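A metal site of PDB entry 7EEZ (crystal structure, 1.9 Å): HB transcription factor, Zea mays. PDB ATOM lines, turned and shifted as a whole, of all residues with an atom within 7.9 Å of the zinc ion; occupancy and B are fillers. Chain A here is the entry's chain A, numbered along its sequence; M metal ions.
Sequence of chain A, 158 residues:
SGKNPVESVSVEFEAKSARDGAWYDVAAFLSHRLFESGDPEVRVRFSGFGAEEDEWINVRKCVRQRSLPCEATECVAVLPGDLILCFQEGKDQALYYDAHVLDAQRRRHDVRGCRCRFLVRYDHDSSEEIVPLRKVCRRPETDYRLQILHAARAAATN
The zinc ion is bound by NE2 of His 109 (2.2 Å), SG of Cys 116 (2.2 Å), SG of Cys 75 (2.4 Å) and SG of Cys 114 (2.4 Å). The zinc ion has four donor atoms within binding distance.
The nearest printed residue that does not touch the zinc ion is Arg 115 (4.1 Å).
SG of Cys 116 lies close to N of Arg 107 (3.6 Å). O of Cys 75 is in hydrogen-bond range of NH1 of Arg 106, at 3.0 Å. O of Ala 72 sits close to SG of Cys 75 (3.6 Å).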
ATOM      1  N   GLU A  71      33.869  12.455   0.008  1.00  0.00           N
ATOM      2  CA  GLU A  71      34.004  11.315  -0.878  1.00  0.00           C
ATOM      3  C   GLU A  71      32.707  11.237  -1.686  1.00  0.00           C
ATOM      4  O   GLU A  71      31.677  11.754  -1.256  1.00  0.00           O
ATOM      5  CB  GLU A  71      34.275  10.030  -0.104  1.00  0.00           C
ATOM      6  CG  GLU A  71      35.627  10.023   0.603  1.00  0.00           C
ATOM      7  CD  GLU A  71      35.689   9.055   1.763  1.00  0.00           C
ATOM      8  OE1 GLU A  71      34.998   8.017   1.722  1.00  0.00           O
ATOM      9  OE2 GLU A  71      36.436   9.335   2.725  1.00  0.00           O
ATOM     10  N   ALA A  72      32.770  10.585  -2.843  1.00  0.00           N
ATOM     11  CA  ALA A  72      31.669  10.610  -3.804  1.00  0.00           C
ATOM     12  C   ALA A  72      30.319  10.202  -3.214  1.00  0.00           C
ATOM     13  O   ALA A  72      29.274  10.689  -3.657  1.00  0.00           O
ATOM     14  CB  ALA A  72      31.997   9.713  -4.990  1.00  0.00           C
ATOM     15  N   THR A  73      30.339   9.334  -2.209  1.00  0.00           N
ATOM     16  CA  THR A  73      29.112   8.823  -1.619  1.00  0.00           C
ATOM     17  C   THR A  73      28.478   9.777  -0.606  1.00  0.00           C
ATOM     18  O   THR A  73      27.358   9.557  -0.151  1.00  0.00           O
ATOM     19  CB  THR A  73      29.356   7.464  -0.941  1.00  0.00           C
ATOM     20  OG1 THR A  73      30.459   7.574  -0.031  1.00  0.00           O
ATOM     21  CG2 THR A  73      29.665   6.394  -1.968  1.00  0.00           C
ATOM     22  N   GLU A  74      29.191  10.844  -0.258  1.00  0.00           N
ATOM     23  CA  GLU A  74      28.746  11.744   0.800  1.00  0.00           C
ATOM     24  C   GLU A  74      27.738  12.794   0.333  1.00  0.00           C
ATOM     25  O   GLU A  74      27.186  13.532   1.153  1.00  0.00           O
ATOM     26  CB  GLU A  74      29.937  12.439   1.447  1.00  0.00           C
ATOM     27  CG  GLU A  74      30.907  11.531   2.159  1.00  0.00           C
ATOM     28  CD  GLU A  74      32.015  12.306   2.845  1.00  0.00           C
ATOM     29  OE1 GLU A  74      31.751  13.453   3.279  1.00  0.00           O
ATOM     30  OE2 GLU A  74      33.138  11.779   2.952  1.00  0.00           O
ATOM     31  N   CYS A  75      27.511  12.864  -0.971  1.00  0.00           N
ATOM     32  CA  CYS A  75      26.646  13.895  -1.552  1.00  0.00           C
ATOM     33  C   CYS A  75      25.215  13.846  -1.020  1.00  0.00           C
ATOM     34  O   CYS A  75      24.523  14.869  -0.999  1.00  0.00           O
ATOM     35  CB  CYS A  75      26.627  13.779  -3.065  1.00  0.00           C
ATOM     36  SG  CYS A  75      25.966  12.212  -3.660  1.00  0.00           S
ATOM     37  N   VAL A  76      24.774  12.675  -0.582  1.00  0.00           N
ATOM     38  CA  VAL A  76      23.409  12.518  -0.081  1.00  0.00           C
ATOM     39  C   VAL A  76      23.247  13.188   1.289  1.00  0.00           C
ATOM     40  O   VAL A  76      22.131  13.394   1.753  1.00  0.00           O
ATOM     41  CB  VAL A  76      23.011  11.040   0.030  1.00  0.00           C
ATOM     42  CG1 VAL A  76      23.114  10.372  -1.325  1.00  0.00           C
ATOM     43  CG2 VAL A  76      23.887  10.324   1.048  1.00  0.00           C
ATOM     44  N   GLN A 105      20.936  19.238  -7.365  1.00  0.00           N
ATOM     45  CA  GLN A 105      20.596  18.440  -8.526  1.00  0.00           C
ATOM     46  C   GLN A 105      21.238  17.067  -8.440  1.00  0.00           C
ATOM     47  O   GLN A 105      22.426  16.901  -8.740  1.00  0.00           O
ATOM     48  CB  GLN A 105      21.009  19.126  -9.817  1.00  0.00           C
ATOM     49  CG  GLN A 105      20.661  18.326 -11.051  1.00  0.00           C
ATOM     50  CD  GLN A 105      21.094  19.014 -12.315  1.00  0.00           C
ATOM     51  OE1 GLN A 105      22.194  19.554 -12.376  1.00  0.00           O
ATOM     52  NE2 GLN A 105      20.250  18.990 -13.335  1.00  0.00           N
ATOM     53  N   ARG A 106      20.450  16.075  -8.027  1.00  0.00           N
ATOM     54  CA  ARG A 106      20.918  14.709  -7.917  1.00  0.00           C
ATOM     55  C   ARG A 106      21.132  14.103  -9.301  1.00  0.00           C
ATOM     56  O   ARG A 106      20.267  14.208 -10.170  1.00  0.00           O
ATOM     57  CB  ARG A 106      19.925  13.865  -7.123  1.00  0.00           C
ATOM     58  CG  ARG A 106      19.410  14.544  -5.858  1.00  0.00           C
ATOM     59  CD  ARG A 106      20.540  14.805  -4.881  1.00  0.00           C
ATOM     60  NE  ARG A 106      20.064  15.476  -3.670  1.00  0.00           N
ATOM     61  CZ  ARG A 106      20.851  15.801  -2.636  1.00  0.00           C
ATOM     62  NH1 ARG A 106      22.142  15.510  -2.677  1.00  0.00           N
ATOM     63  NH2 ARG A 106      20.337  16.404  -1.586  1.00  0.00           N
ATOM     64  N   ARG A 107      22.283  13.461  -9.498  1.00  0.00           N
ATOM     65  CA  ARG A 107      22.571  12.739 -10.742  1.00  0.00           C
ATOM     66  C   ARG A 107      23.288  11.414 -10.463  1.00  0.00           C
ATOM     67  O   ARG A 107      24.172  11.366  -9.605  1.00  0.00           O
ATOM     68  CB  ARG A 107      23.426  13.596 -11.671  1.00  0.00           C
ATOM     69  CG  ARG A 107      22.730  14.820 -12.241  1.00  0.00           C
ATOM     70  CD  ARG A 107      23.757  15.785 -12.806  1.00  0.00           C
ATOM     71  NE  ARG A 107      23.210  16.629 -13.857  1.00  0.00           N
ATOM     72  CZ  ARG A 107      23.958  17.359 -14.688  1.00  0.00           C
ATOM     73  NH1 ARG A 107      25.274  17.353 -14.559  1.00  0.00           N
ATOM     74  NH2 ARG A 107      23.384  18.097 -15.619  1.00  0.00           N
ATOM     75  N   ARG A 108      22.896  10.363 -11.175  1.00  0.00           N
ATOM     76  CA  ARG A 108      23.557   9.064 -11.104  1.00  0.00           C
ATOM     77  C   ARG A 108      25.044   9.259 -11.320  1.00  0.00           C
ATOM     78  O   ARG A 108      25.455   9.970 -12.227  1.00  0.00           O
ATOM     79  CB  ARG A 108      23.001   8.087 -12.149  1.00  0.00           C
ATOM     80  CG  ARG A 108      23.359   6.587 -11.968  1.00  0.00           C
ATOM     81  CD  ARG A 108      23.609   6.160 -10.503  1.00  0.00           C
ATOM     82  NE  ARG A 108      24.121   4.798 -10.406  1.00  0.00           N
ATOM     83  CZ  ARG A 108      25.417   4.497 -10.327  1.00  0.00           C
ATOM     84  NH1 ARG A 108      26.333   5.446 -10.331  1.00  0.00           N
ATOM     85  NH2 ARG A 108      25.796   3.229 -10.241  1.00  0.00           N
ATOM     86  N   HIS A 109      25.837   8.669 -10.445  1.00  0.00           N
ATOM     87  CA  HIS A 109      27.277   8.785 -10.502  1.00  0.00           C
ATOM     88  C   HIS A 109      27.800   7.944 -11.659  1.00  0.00           C
ATOM     89  O   HIS A 109      27.095   7.075 -12.187  1.00  0.00           O
ATOM     90  CB  HIS A 109      27.903   8.309  -9.199  1.00  0.00           C
ATOM     91  CG  HIS A 109      27.524   9.122  -8.006  1.00  0.00           C
ATOM     92  ND1 HIS A 109      28.057   8.916  -6.757  1.00  0.00           N
ATOM     93  CD2 HIS A 109      26.644  10.157  -7.872  1.00  0.00           C
ATOM     94  CE1 HIS A 109      27.541   9.778  -5.902  1.00  0.00           C
ATOM     95  NE2 HIS A 109      26.682  10.540  -6.550  1.00  0.00           N
ATOM     96  N   GLY A 113      32.918   9.292 -10.214  1.00  0.00           N
ATOM     97  CA  GLY A 113      32.442   9.684  -8.905  1.00  0.00           C
ATOM     98  C   GLY A 113      31.111  10.405  -8.953  1.00  0.00           C
ATOM     99  O   GLY A 113      30.274  10.120  -9.808  1.00  0.00           O
ATOM    100  N   CYS A 114      30.922  11.348  -8.037  1.00  0.00           N
ATOM    101  CA  CYS A 114      29.659  12.079  -7.919  1.00  0.00           C
ATOM    102  C   CYS A 114      29.419  13.026  -9.091  1.00  0.00           C
ATOM    103  O   CYS A 114      30.318  13.748  -9.524  1.00  0.00           O
ATOM    104  CB  CYS A 114      29.647  12.872  -6.599  1.00  0.00           C
ATOM    105  SG  CYS A 114      28.240  13.985  -6.399  1.00  0.00           S
ATOM    106  N   ARG A 115      28.190  13.006  -9.620  1.00  0.00           N
ATOM    107  CA  ARG A 115      27.814  13.890 -10.723  1.00  0.00           C
ATOM    108  C   ARG A 115      26.870  14.989 -10.275  1.00  0.00           C
ATOM    109  O   ARG A 115      26.421  15.799 -11.084  1.00  0.00           O
ATOM    110  CB  ARG A 115      27.177  13.095 -11.860  1.00  0.00           C
ATOM    111  CG  ARG A 115      28.167  12.450 -12.811  1.00  0.00           C
ATOM    112  CD  ARG A 115      27.486  11.799 -14.004  1.00  0.00           C
ATOM    113  NE  ARG A 115      26.936  12.789 -14.933  1.00  0.00           N
ATOM    114  CZ  ARG A 115      25.641  12.974 -15.157  1.00  0.00           C
ATOM    115  NH1 ARG A 115      24.745  12.230 -14.519  1.00  0.00           N
ATOM    116  NH2 ARG A 115      25.235  13.898 -16.016  1.00  0.00           N
ATOM    117  N   CYS A 116      26.562  15.012  -8.980  1.00  0.00           N
ATOM    118  CA  CYS A 116      25.606  15.980  -8.459  1.00  0.00           C
ATOM    119  C   CYS A 116      26.144  17.401  -8.533  1.00  0.00           C
ATOM    120  O   CYS A 116      27.349  17.627  -8.439  1.00  0.00           O
ATOM    121  CB  CYS A 116      25.229  15.628  -7.019  1.00  0.00           C
ATOM    122  SG  CYS A 116      24.711  13.913  -6.816  1.00  0.00           S
ATOM    123  N   ARG A 117      25.241  18.350  -8.719  1.00  0.00           N
ATOM    124  CA  ARG A 117      25.602  19.764  -8.683  1.00  0.00           C
ATOM    125  C   ARG A 117      24.750  20.468  -7.638  1.00  0.00           C
ATOM    126  O   ARG A 117      23.619  20.061  -7.367  1.00  0.00           O
ATOM    127  CB  ARG A 117      25.443  20.421 -10.058  1.00  0.00           C
ATOM    128  CG  ARG A 117      26.360  19.841 -11.137  1.00  0.00           C
ATOM    129  CD  ARG A 117      26.111  20.446 -12.517  1.00  0.00           C
ATOM    130  NE  ARG A 117      24.723  20.842 -12.721  1.00  0.00           N
ATOM    131  CZ  ARG A 117      24.175  21.039 -13.915  1.00  0.00           C
ATOM    132  NH1 ARG A 117      24.883  20.852 -15.018  1.00  0.00           N
ATOM    133  NH2 ARG A 117      22.898  21.414 -14.008  1.00  0.00           N
ATOM    134  N   PHE A 118      25.296  21.531  -7.056  1.00  0.00           N
ATOM    135  CA  PHE A 118      24.634  22.236  -5.966  1.00  0.00           C
ATOM    136  C   PHE A 118      24.588  23.726  -6.223  1.00  0.00           C
ATOM    137  O   PHE A 118      25.629  24.367  -6.414  1.00  0.00           O
ATOM    138  CB  PHE A 118      25.353  21.961  -4.638  1.00  0.00           C
ATOM    139  CG  PHE A 118      25.457  20.514  -4.296  1.00  0.00           C
ATOM    140  CD1 PHE A 118      26.565  19.770  -4.666  1.00  0.00           C
ATOM    141  CD2 PHE A 118      24.445  19.891  -3.589  1.00  0.00           C
ATOM    142  CE1 PHE A 118      26.657  18.434  -4.353  1.00  0.00           C
ATOM    143  CE2 PHE A 118      24.535  18.546  -3.266  1.00  0.00           C
ATOM    144  CZ  PHE A 118      25.650  17.825  -3.643  1.00  0.00           C
ATOM    145  N   LEU A 133      30.562  18.520  -6.176  1.00  0.00           N
ATOM    146  CA  LEU A 133      30.865  18.038  -4.834  1.00  0.00           C
ATOM    147  C   LEU A 133      32.284  18.393  -4.394  1.00  0.00           C
ATOM    148  O   LEU A 133      32.550  18.572  -3.212  1.00  0.00           O
ATOM    149  CB  LEU A 133      30.668  16.525  -4.766  1.00  0.00           C
ATOM    150  CG  LEU A 133      30.682  15.925  -3.361  1.00  0.00           C
ATOM    151  CD1 LEU A 133      29.475  16.401  -2.568  1.00  0.00           C
ATOM    152  CD2 LEU A 133      30.721  14.397  -3.424  1.00  0.00           C
HETATM  153 ZN    ZN M   1      26.327  12.637  -5.950  1.00  0.00          ZN
